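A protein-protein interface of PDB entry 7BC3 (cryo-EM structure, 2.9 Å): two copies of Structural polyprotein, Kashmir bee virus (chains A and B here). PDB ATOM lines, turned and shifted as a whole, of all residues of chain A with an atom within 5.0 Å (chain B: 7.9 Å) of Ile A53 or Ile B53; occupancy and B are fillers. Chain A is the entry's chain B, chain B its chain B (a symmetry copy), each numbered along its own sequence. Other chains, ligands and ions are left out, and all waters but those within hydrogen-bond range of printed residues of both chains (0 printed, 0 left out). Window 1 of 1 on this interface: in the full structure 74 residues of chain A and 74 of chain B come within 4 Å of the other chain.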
ATOM      1  N   HIS A  51       6.864 -30.293  -3.620  1.00  0.00           N
ATOM      2  CA  HIS A  51       6.643 -29.061  -4.360  1.00  0.00           C
ATOM      3  C   HIS A  51       5.603 -28.202  -3.655  1.00  0.00           C
ATOM      4  O   HIS A  51       4.509 -28.673  -3.334  1.00  0.00           O
ATOM      5  CB  HIS A  51       6.198 -29.377  -5.786  1.00  0.00           C
ATOM      6  CG  HIS A  51       7.266 -30.006  -6.622  1.00  0.00           C
ATOM      7  ND1 HIS A  51       6.990 -30.753  -7.746  1.00  0.00           N
ATOM      8  CD2 HIS A  51       8.614 -29.998  -6.498  1.00  0.00           C
ATOM      9  CE1 HIS A  51       8.121 -31.178  -8.278  1.00  0.00           C
ATOM     10  NE2 HIS A  51       9.122 -30.734  -7.540  1.00  0.00           N
ATOM     11  N   SER A  52       5.954 -26.943  -3.415  1.00  0.00           N
ATOM     12  CA  SER A  52       5.030 -26.003  -2.810  1.00  0.00           C
ATOM     13  C   SER A  52       3.928 -25.634  -3.801  1.00  0.00           C
ATOM     14  O   SER A  52       3.955 -26.005  -4.977  1.00  0.00           O
ATOM     15  CB  SER A  52       5.771 -24.749  -2.353  1.00  0.00           C
ATOM     16  OG  SER A  52       6.458 -24.143  -3.432  1.00  0.00           O
ATOM     17  N   ILE A  53       2.939 -24.888  -3.306  1.00  0.00           N
ATOM     18  CA  ILE A  53       1.871 -24.413  -4.180  1.00  0.00           C
ATOM     19  C   ILE A  53       2.440 -23.485  -5.242  1.00  0.00           C
ATOM     20  O   ILE A  53       2.042 -23.535  -6.412  1.00  0.00           O
ATOM     21  CB  ILE A  53       0.771 -23.722  -3.355  1.00  0.00           C
ATOM     22  CG1 ILE A  53       0.071 -24.730  -2.446  1.00  0.00           C
ATOM     23  CG2 ILE A  53      -0.238 -23.068  -4.272  1.00  0.00           C
ATOM     24  CD1 ILE A  53      -0.724 -24.096  -1.332  1.00  0.00           C
ATOM     25  N   ILE A  54       3.380 -22.623  -4.852  1.00  0.00           N
ATOM     26  CA  ILE A  54       4.031 -21.740  -5.814  1.00  0.00           C
ATOM     27  C   ILE A  54       4.637 -22.553  -6.951  1.00  0.00           C
ATOM     28  O   ILE A  54       4.360 -22.308  -8.130  1.00  0.00           O
ATOM     29  CB  ILE A  54       5.094 -20.879  -5.110  1.00  0.00           C
ATOM     30  CG1 ILE A  54       4.420 -19.829  -4.228  1.00  0.00           C
ATOM     31  CG2 ILE A  54       6.011 -20.226  -6.128  1.00  0.00           C
ATOM     32  CD1 ILE A  54       5.375 -19.079  -3.336  1.00  0.00           C
ATOM     33  N   GLN A  55       5.478 -23.530  -6.610  1.00  0.00           N
ATOM     34  CA  GLN A  55       6.089 -24.371  -7.633  1.00  0.00           C
ATOM     35  C   GLN A  55       5.032 -25.016  -8.518  1.00  0.00           C
ATOM     36  O   GLN A  55       5.188 -25.074  -9.742  1.00  0.00           O
ATOM     37  CB  GLN A  55       6.958 -25.439  -6.975  1.00  0.00           C
ATOM     38  CG  GLN A  55       8.149 -24.885  -6.226  1.00  0.00           C
ATOM     39  CD  GLN A  55       9.030 -25.973  -5.652  1.00  0.00           C
ATOM     40  OE1 GLN A  55       9.218 -27.023  -6.264  1.00  0.00           O
ATOM     41  NE2 GLN A  55       9.576 -25.727  -4.469  1.00  0.00           N
ATOM     42  N   PHE A  56       3.952 -25.512  -7.914  1.00  0.00           N
ATOM     43  CA  PHE A  56       2.875 -26.106  -8.698  1.00  0.00           C
ATOM     44  C   PHE A  56       2.300 -25.105  -9.688  1.00  0.00           C
ATOM     45  O   PHE A  56       1.918 -25.472 -10.805  1.00  0.00           O
ATOM     46  CB  PHE A  56       1.784 -26.624  -7.765  1.00  0.00           C
ATOM     47  CG  PHE A  56       0.744 -27.457  -8.450  1.00  0.00           C
ATOM     48  CD1 PHE A  56       0.819 -28.834  -8.420  1.00  0.00           C
ATOM     49  CD2 PHE A  56      -0.309 -26.863  -9.117  1.00  0.00           C
ATOM     50  CE1 PHE A  56      -0.135 -29.604  -9.046  1.00  0.00           C
ATOM     51  CE2 PHE A  56      -1.265 -27.628  -9.745  1.00  0.00           C
ATOM     52  CZ  PHE A  56      -1.178 -29.000  -9.709  1.00  0.00           C
ATOM     53  N   LEU A  57       2.229 -23.833  -9.295  1.00  0.00           N
ATOM     54  CA  LEU A  57       1.677 -22.806 -10.167  1.00  0.00           C
ATOM     55  C   LEU A  57       2.678 -22.313 -11.200  1.00  0.00           C
ATOM     56  O   LEU A  57       2.271 -21.701 -12.192  1.00  0.00           O
ATOM     57  CB  LEU A  57       1.181 -21.629  -9.332  1.00  0.00           C
ATOM     58  CG  LEU A  57       0.080 -21.945  -8.323  1.00  0.00           C
ATOM     59  CD1 LEU A  57      -0.192 -20.738  -7.455  1.00  0.00           C
ATOM     60  CD2 LEU A  57      -1.184 -22.406  -9.013  1.00  0.00           C
ATOM     61  N   LYS A 112      -5.437 -25.757  -6.336  1.00  0.00           N
ATOM     62  CA  LYS A 112      -4.439 -25.275  -5.392  1.00  0.00           C
ATOM     63  C   LYS A 112      -4.648 -23.819  -5.005  1.00  0.00           C
ATOM     64  O   LYS A 112      -4.022 -23.353  -4.047  1.00  0.00           O
ATOM     65  CB  LYS A 112      -3.036 -25.453  -5.977  1.00  0.00           C
ATOM     66  CG  LYS A 112      -2.416 -26.799  -5.667  1.00  0.00           C
ATOM     67  CD  LYS A 112      -3.110 -27.895  -6.439  1.00  0.00           C
ATOM     68  CE  LYS A 112      -2.578 -29.265  -6.087  1.00  0.00           C
ATOM     69  NZ  LYS A 112      -3.345 -30.323  -6.788  1.00  0.00           N
ATOM     70  N   PHE A 116      -8.370 -19.883  -0.849  1.00  0.00           N
ATOM     71  CA  PHE A 116      -7.590 -18.664  -0.717  1.00  0.00           C
ATOM     72  C   PHE A 116      -8.400 -17.505  -1.275  1.00  0.00           C
ATOM     73  O   PHE A 116      -9.401 -17.692  -1.972  1.00  0.00           O
ATOM     74  CB  PHE A 116      -6.242 -18.763  -1.438  1.00  0.00           C
ATOM     75  CG  PHE A 116      -5.229 -19.596  -0.717  1.00  0.00           C
ATOM     76  CD1 PHE A 116      -4.522 -19.075   0.349  1.00  0.00           C
ATOM     77  CD2 PHE A 116      -4.976 -20.896  -1.109  1.00  0.00           C
ATOM     78  CE1 PHE A 116      -3.588 -19.837   1.013  1.00  0.00           C
ATOM     79  CE2 PHE A 116      -4.043 -21.662  -0.449  1.00  0.00           C
ATOM     80  CZ  PHE A 116      -3.348 -21.132   0.614  1.00  0.00           C
ATOM     81  N   GLN B  20      10.284 -25.858 -13.470  1.00  0.00           N
ATOM     82  CA  GLN B  20       9.690 -26.328 -12.224  1.00  0.00           C
ATOM     83  C   GLN B  20       8.980 -27.672 -12.324  1.00  0.00           C
ATOM     84  O   GLN B  20       8.792 -28.355 -11.311  1.00  0.00           O
ATOM     85  CB  GLN B  20       8.686 -25.278 -11.740  1.00  0.00           C
ATOM     86  CG  GLN B  20       8.228 -25.455 -10.327  1.00  0.00           C
ATOM     87  CD  GLN B  20       9.356 -25.360  -9.338  1.00  0.00           C
ATOM     88  OE1 GLN B  20       9.945 -24.304  -9.153  1.00  0.00           O
ATOM     89  NE2 GLN B  20       9.674 -26.473  -8.696  1.00  0.00           N
ATOM     90  N   THR B  50       2.903 -16.894   2.366  1.00  0.00           N
ATOM     91  CA  THR B  50       2.304 -17.844   1.441  1.00  0.00           C
ATOM     92  C   THR B  50       2.480 -19.253   1.991  1.00  0.00           C
ATOM     93  O   THR B  50       3.606 -19.686   2.264  1.00  0.00           O
ATOM     94  CB  THR B  50       2.933 -17.720   0.057  1.00  0.00           C
ATOM     95  OG1 THR B  50       2.807 -16.372  -0.407  1.00  0.00           O
ATOM     96  CG2 THR B  50       2.246 -18.651  -0.924  1.00  0.00           C
ATOM     97  N   HIS B  51       1.371 -19.965   2.150  1.00  0.00           N
ATOM     98  CA  HIS B  51       1.370 -21.265   2.802  1.00  0.00           C
ATOM     99  C   HIS B  51       1.625 -22.366   1.782  1.00  0.00           C
ATOM    100  O   HIS B  51       0.952 -22.439   0.750  1.00  0.00           O
ATOM    101  CB  HIS B  51       0.039 -21.496   3.513  1.00  0.00           C
ATOM    102  CG  HIS B  51      -0.171 -20.603   4.695  1.00  0.00           C
ATOM    103  ND1 HIS B  51      -1.419 -20.325   5.207  1.00  0.00           N
ATOM    104  CD2 HIS B  51       0.711 -19.924   5.466  1.00  0.00           C
ATOM    105  CE1 HIS B  51      -1.298 -19.515   6.242  1.00  0.00           C
ATOM    106  NE2 HIS B  51      -0.015 -19.256   6.420  1.00  0.00           N
ATOM    107  N   SER B  52       2.604 -23.216   2.075  1.00  0.00           N
ATOM    108  CA  SER B  52       2.903 -24.348   1.220  1.00  0.00           C
ATOM    109  C   SER B  52       1.797 -25.397   1.323  1.00  0.00           C
ATOM    110  O   SER B  52       0.879 -25.299   2.142  1.00  0.00           O
ATOM    111  CB  SER B  52       4.248 -24.961   1.599  1.00  0.00           C
ATOM    112  OG  SER B  52       4.261 -25.351   2.961  1.00  0.00           O
ATOM    113  N   ILE B  53       1.893 -26.416   0.470  1.00  0.00           N
ATOM    114  CA  ILE B  53       0.934 -27.515   0.530  1.00  0.00           C
ATOM    115  C   ILE B  53       1.045 -28.234   1.865  1.00  0.00           C
ATOM    116  O   ILE B  53       0.037 -28.616   2.470  1.00  0.00           O
ATOM    117  CB  ILE B  53       1.148 -28.478  -0.651  1.00  0.00           C
ATOM    118  CG1 ILE B  53       0.820 -27.786  -1.973  1.00  0.00           C
ATOM    119  CG2 ILE B  53       0.283 -29.709  -0.486  1.00  0.00           C
ATOM    120  CD1 ILE B  53       1.372 -28.495  -3.184  1.00  0.00           C
ATOM    121  N   ILE B  54       2.274 -28.428   2.346  1.00  0.00           N
ATOM    122  CA  ILE B  54       2.477 -29.049   3.651  1.00  0.00           C
ATOM    123  C   ILE B  54       1.710 -28.286   4.724  1.00  0.00           C
ATOM    124  O   ILE B  54       0.913 -28.862   5.471  1.00  0.00           O
ATOM    125  CB  ILE B  54       3.979 -29.122   3.977  1.00  0.00           C
ATOM    126  CG1 ILE B  54       4.658 -30.171   3.097  1.00  0.00           C
ATOM    127  CG2 ILE B  54       4.190 -29.428   5.448  1.00  0.00           C
ATOM    128  CD1 ILE B  54       6.161 -30.164   3.193  1.00  0.00           C
ATOM    129  N   GLN B  55       1.948 -26.977   4.816  1.00  0.00           N
ATOM    130  CA  GLN B  55       1.245 -26.165   5.800  1.00  0.00           C
ATOM    131  C   GLN B  55      -0.264 -26.308   5.657  1.00  0.00           C
ATOM    132  O   GLN B  55      -0.983 -26.423   6.654  1.00  0.00           O
ATOM    133  CB  GLN B  55       1.658 -24.703   5.658  1.00  0.00           C
ATOM    134  CG  GLN B  55       3.113 -24.442   5.973  1.00  0.00           C
ATOM    135  CD  GLN B  55       3.470 -22.974   5.896  1.00  0.00           C
ATOM    136  OE1 GLN B  55       2.676 -22.111   6.263  1.00  0.00           O
ATOM    137  NE2 GLN B  55       4.670 -22.683   5.414  1.00  0.00           N
ATOM    138  N   PHE B  56      -0.760 -26.297   4.420  1.00  0.00           N
ATOM    139  CA  PHE B  56      -2.190 -26.474   4.196  1.00  0.00           C
ATOM    140  C   PHE B  56      -2.675 -27.801   4.760  1.00  0.00           C
ATOM    141  O   PHE B  56      -3.795 -27.896   5.274  1.00  0.00           O
ATOM    142  CB  PHE B  56      -2.494 -26.385   2.703  1.00  0.00           C
ATOM    143  CG  PHE B  56      -3.956 -26.322   2.383  1.00  0.00           C
ATOM    144  CD1 PHE B  56      -4.567 -25.109   2.138  1.00  0.00           C
ATOM    145  CD2 PHE B  56      -4.716 -27.473   2.321  1.00  0.00           C
ATOM    146  CE1 PHE B  56      -5.910 -25.045   1.841  1.00  0.00           C
ATOM    147  CE2 PHE B  56      -6.058 -27.415   2.026  1.00  0.00           C
ATOM    148  CZ  PHE B  56      -6.656 -26.200   1.786  1.00  0.00           C
ATOM    149  N   LEU B  57      -1.843 -28.839   4.673  1.00  0.00           N
ATOM    150  CA  LEU B  57      -2.224 -30.153   5.170  1.00  0.00           C
ATOM    151  C   LEU B  57      -2.051 -30.284   6.675  1.00  0.00           C
ATOM    152  O   LEU B  57      -2.627 -31.199   7.272  1.00  0.00           O
ATOM    153  CB  LEU B  57      -1.408 -31.232   4.464  1.00  0.00           C
ATOM    154  CG  LEU B  57      -1.569 -31.303   2.947  1.00  0.00           C
ATOM    155  CD1 LEU B  57      -0.584 -32.292   2.367  1.00  0.00           C
ATOM    156  CD2 LEU B  57      -2.985 -31.667   2.561  1.00  0.00           C
ATOM    157  N   GLN B  58      -1.275 -29.400   7.297  1.00  0.00           N
ATOM    158  CA  GLN B  58      -1.146 -29.354   8.745  1.00  0.00           C
ATOM    159  C   GLN B  58      -2.263 -28.565   9.405  1.00  0.00           C
ATOM    160  O   GLN B  58      -2.138 -28.196  10.579  1.00  0.00           O
ATOM    161  CB  GLN B  58       0.200 -28.746   9.135  1.00  0.00           C
ATOM    162  CG  GLN B  58       1.401 -29.559   8.716  1.00  0.00           C
ATOM    163  CD  GLN B  58       2.699 -28.811   8.911  1.00  0.00           C
ATOM    164  OE1 GLN B  58       2.705 -27.606   9.166  1.00  0.00           O
ATOM    165  NE2 GLN B  58       3.811 -29.520   8.795  1.00  0.00           N
ATOM    166  N   ARG B  59      -3.334 -28.301   8.689  1.00  0.00           N
ATOM    167  CA  ARG B  59      -4.426 -27.498   9.216  1.00  0.00           C
ATOM    168  C   ARG B  59      -5.444 -28.394   9.910  1.00  0.00           C
ATOM    169  O   ARG B  59      -5.942 -29.342   9.293  1.00  0.00           O
ATOM    170  CB  ARG B  59      -5.106 -26.726   8.102  1.00  0.00           C
ATOM    171  CG  ARG B  59      -4.326 -25.528   7.623  1.00  0.00           C
ATOM    172  CD  ARG B  59      -5.073 -24.816   6.525  1.00  0.00           C
ATOM    173  NE  ARG B  59      -4.322 -23.697   5.975  1.00  0.00           N
ATOM    174  CZ  ARG B  59      -4.788 -22.884   5.037  1.00  0.00           C
ATOM    175  NH1 ARG B  59      -6.003 -23.066   4.543  1.00  0.00           N
ATOM    176  NH2 ARG B  59      -4.041 -21.889   4.592  1.00  0.00           N
ATOM    177  N   LYS B 109      -8.358 -30.999   1.515  1.00  0.00           N
ATOM    178  CA  LYS B 109      -6.987 -31.461   1.350  1.00  0.00           C
ATOM    179  C   LYS B 109      -6.805 -32.247   0.062  1.00  0.00           C
ATOM    180  O   LYS B 109      -5.734 -32.187  -0.550  1.00  0.00           O
ATOM    181  CB  LYS B 109      -6.588 -32.323   2.546  1.00  0.00           C
ATOM    182  CG  LYS B 109      -6.625 -31.595   3.872  1.00  0.00           C
ATOM    183  CD  LYS B 109      -5.892 -32.375   4.943  1.00  0.00           C
ATOM    184  CE  LYS B 109      -6.131 -31.791   6.320  1.00  0.00           C
ATOM    185  NZ  LYS B 109      -5.918 -30.325   6.356  1.00  0.00           N
ATOM    186  N   GLN B 111      -7.909 -31.629  -2.778  1.00  0.00           N
ATOM    187  CA  GLN B 111      -7.606 -30.711  -3.869  1.00  0.00           C
ATOM    188  C   GLN B 111      -6.117 -30.410  -3.947  1.00  0.00           C
ATOM    189  O   GLN B 111      -5.584 -30.205  -5.043  1.00  0.00           O
ATOM    190  CB  GLN B 111      -8.395 -29.417  -3.691  1.00  0.00           C
ATOM    191  CG  GLN B 111      -9.895 -29.591  -3.783  1.00  0.00           C
ATOM    192  CD  GLN B 111     -10.619 -28.275  -3.967  1.00  0.00           C
ATOM    193  OE1 GLN B 111     -10.459 -27.603  -4.985  1.00  0.00           O
ATOM    194  NE2 GLN B 111     -11.416 -27.896  -2.977  1.00  0.00           N
ATOM    195  N   LYS B 112      -5.433 -30.376  -2.808  1.00  0.00           N
ATOM    196  CA  LYS B 112      -4.002 -30.111  -2.776  1.00  0.00           C
ATOM    197  C   LYS B 112      -3.166 -31.375  -2.911  1.00  0.00           C
ATOM    198  O   LYS B 112      -1.954 -31.276  -3.130  1.00  0.00           O
ATOM    199  CB  LYS B 112      -3.632 -29.389  -1.478  1.00  0.00           C
ATOM    200  CG  LYS B 112      -3.726 -27.881  -1.577  1.00  0.00           C
ATOM    201  CD  LYS B 112      -5.168 -27.441  -1.663  1.00  0.00           C
ATOM    202  CE  LYS B 112      -5.299 -25.948  -1.853  1.00  0.00           C
ATOM    203  NZ  LYS B 112      -6.719 -25.562  -2.032  1.00  0.00           N
ATOM    204  N   LEU B 113      -3.778 -32.548  -2.784  1.00  0.00           N
ATOM    205  CA  LEU B 113      -3.103 -33.805  -3.072  1.00  0.00           C
ATOM    206  C   LEU B 113      -3.267 -34.230  -4.520  1.00  0.00           C
ATOM    207  O   LEU B 113      -2.441 -34.998  -5.024  1.00  0.00           O
ATOM    208  CB  LEU B 113      -3.642 -34.918  -2.177  1.00  0.00           C
ATOM    209  CG  LEU B 113      -3.581 -34.693  -0.669  1.00  0.00           C
ATOM    210  CD1 LEU B 113      -4.529 -35.643   0.020  1.00  0.00           C
ATOM    211  CD2 LEU B 113      -2.170 -34.880  -0.157  1.00  0.00           C
ATOM    212  N   ALA B 114      -4.317 -33.760  -5.188  1.00  0.00           N
ATOM    213  CA  ALA B 114      -4.540 -34.096  -6.583  1.00  0.00           C
ATOM    214  C   ALA B 114      -3.277 -33.848  -7.398  1.00  0.00           C
ATOM    215  O   ALA B 114      -2.458 -32.988  -7.069  1.00  0.00           O
ATOM    216  CB  ALA B 114      -5.695 -33.271  -7.143  1.00  0.00           C
ATOM    217  N   PHE B 116      -0.785 -35.723  -7.606  1.00  0.00           N
ATOM    218  CA  PHE B 116       0.358 -36.350  -6.965  1.00  0.00           C
ATOM    219  C   PHE B 116       0.089 -37.841  -6.841  1.00  0.00           C
ATOM    220  O   PHE B 116      -1.041 -38.310  -7.000  1.00  0.00           O
ATOM    221  CB  PHE B 116       0.647 -35.747  -5.587  1.00  0.00           C
ATOM    222  CG  PHE B 116       1.300 -34.403  -5.638  1.00  0.00           C
ATOM    223  CD1 PHE B 116       2.656 -34.290  -5.876  1.00  0.00           C
ATOM    224  CD2 PHE B 116       0.563 -33.252  -5.441  1.00  0.00           C
ATOM    225  CE1 PHE B 116       3.262 -33.054  -5.921  1.00  0.00           C
ATOM    226  CE2 PHE B 116       1.163 -32.014  -5.486  1.00  0.00           C
ATOM    227  CZ  PHE B 116       2.514 -31.915  -5.725  1.00  0.00           C
ATOM    228  N   LEU B 233      -2.370 -33.547   9.390  1.00  0.00           N
ATOM    229  CA  LEU B 233      -1.254 -34.400   9.020  1.00  0.00           C
ATOM    230  C   LEU B 233       0.053 -33.806   9.523  1.00  0.00           C
ATOM    231  O   LEU B 233       0.139 -32.622   9.860  1.00  0.00           O
ATOM    232  CB  LEU B 233      -1.184 -34.593   7.503  1.00  0.00           C
ATOM    233  CG  LEU B 233      -2.467 -35.054   6.814  1.00  0.00           C
ATOM    234  CD1 LEU B 233      -2.255 -35.104   5.321  1.00  0.00           C
ATOM    235  CD2 LEU B 233      -2.910 -36.403   7.339  1.00  0.00           C
ATOM    236  N   ILE B 236       5.135 -34.641   6.305  1.00  0.00           N
ATOM    237  CA  ILE B 236       4.502 -34.841   5.007  1.00  0.00           C
ATOM    238  C   ILE B 236       5.553 -34.860   3.908  1.00  0.00           C
ATOM    239  O   ILE B 236       6.625 -34.261   4.028  1.00  0.00           O
ATOM    240  CB  ILE B 236       3.451 -33.742   4.751  1.00  0.00           C
ATOM    241  CG1 ILE B 236       2.321 -33.847   5.770  1.00  0.00           C
ATOM    242  CG2 ILE B 236       2.893 -33.842   3.348  1.00  0.00           C
ATOM    243  CD1 ILE B 236       1.760 -32.520   6.177  1.00  0.00           C
ATOM    244  N   LEU B 238       4.987 -34.960  -0.439  1.00  0.00           N
ATOM    245  CA  LEU B 238       4.365 -35.168  -1.742  1.00  0.00           C
ATOM    246  C   LEU B 238       5.450 -35.007  -2.797  1.00  0.00           C
ATOM    247  O   LEU B 238       6.107 -33.962  -2.852  1.00  0.00           O
ATOM    248  CB  LEU B 238       3.234 -34.169  -1.987  1.00  0.00           C
ATOM    249  CG  LEU B 238       1.842 -34.476  -1.437  1.00  0.00           C
ATOM    250  CD1 LEU B 238       1.228 -35.698  -2.102  1.00  0.00           C
ATOM    251  CD2 LEU B 238       1.903 -34.648   0.062  1.00  0.00           C
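The guanidinium group of Arg B59 is in hydrogen-bond range of a ring nitrogen (ND1) of His B51 (3.1 Å).
The backbone NH (N) of Gln A55 lies close to the side-chain hydroxyl (OG) of Ser A52, 3.4 Å away.
OG of Ser B52 sits close to N of Gln B55 (3.4 Å).
Hydrophobic or aromatic side chains of chain B within 4 Å of the printed part of chain A: Ile B53 and Ala B114.
Of the 9 printed residues of chain A, 6 touch a printed residue of chain B.
Printed residues of chain A that touch a printed residue of chain B: His A51, Ser A52, Ile A53, Ile A54, Gln A55 and Lys A112.
Among the printed residues, 11 pairs touch across the chains.
Of chain B, only His B51 (3.1 Å), Ser B52 (3.9 Å) and Ile B53 (3.2 Å) come within 4 Å of Ile A53.
Of chain A, only His A51 (3.1 Å), Ser A52 (3.9 Å) and Ile A53 (3.2 Å) come within 4 Å of Ile B53.
Ser A52 touches just one residue of chain B: Ile B53 (3.9 Å).
Of the printed residues of chain A, Ser B52 touches Ile A53.
Of the printed residues of chain B, Lys A112 touches Gln B111 (2.8 Å), Lys B112 (3.6 Å) and Ala B114 (2.8 Å).
Of the printed residues of chain A, Gln B20 touches Gln A55.
Of the printed residues of chain A, His B51 touches Ile A53.
Of the printed residues of chain B, Gln A55 touches Gln B20.
Phe B56 touches none of the printed residues of chain A.
The nearest residue of chain B that does not touch Ile A53 is Lys B112 (4.8 Å).
The nearest residue of chain A that does not touch Ile B53 is Lys A112 (4.8 Å).
The nearest printed residue of chain A that does not touch Gln B20 is His A51 (4.2 Å).
The side-chain amino group (NZ) of Lys A112 sits at hydrogen-bond distance from the backbone carbonyl oxygen (O) of Gln B111, 2.8 Å away.
OE1 of Gln A55 is in hydrogen-bond range of NE2 of Gln B20, at 2.5 Å.
The side-chain amino group of Lys A112 is in hydrogen-bond range of the backbone carbonyl oxygen of Ala B114 (2.8 Å).
His A51 touches Ile B53, and with the chains exchanged Ile A53 touches His B51.
Ser A52 touches Ile B53, and with the chains exchanged Ile A53 touches Ser B52.
Ile B53 touches its own counterpart, Ile A53.
Lys B112 touches its own counterpart, Lys A112.
Positions printed for both chains: 51, 52, 53, 54, 55, 56, 57, 112 and 116.
Among the printed residues, merely in contact across the chains: His A51 with Ile B53, His A51 with Leu B238, Ser A52 with Ile B53, Ile A53 with His B51, Ile A53 with Ser B52, Ile A53 with Ile B53, Ile A54 with Thr B50 and Lys A112 with Lys B112.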
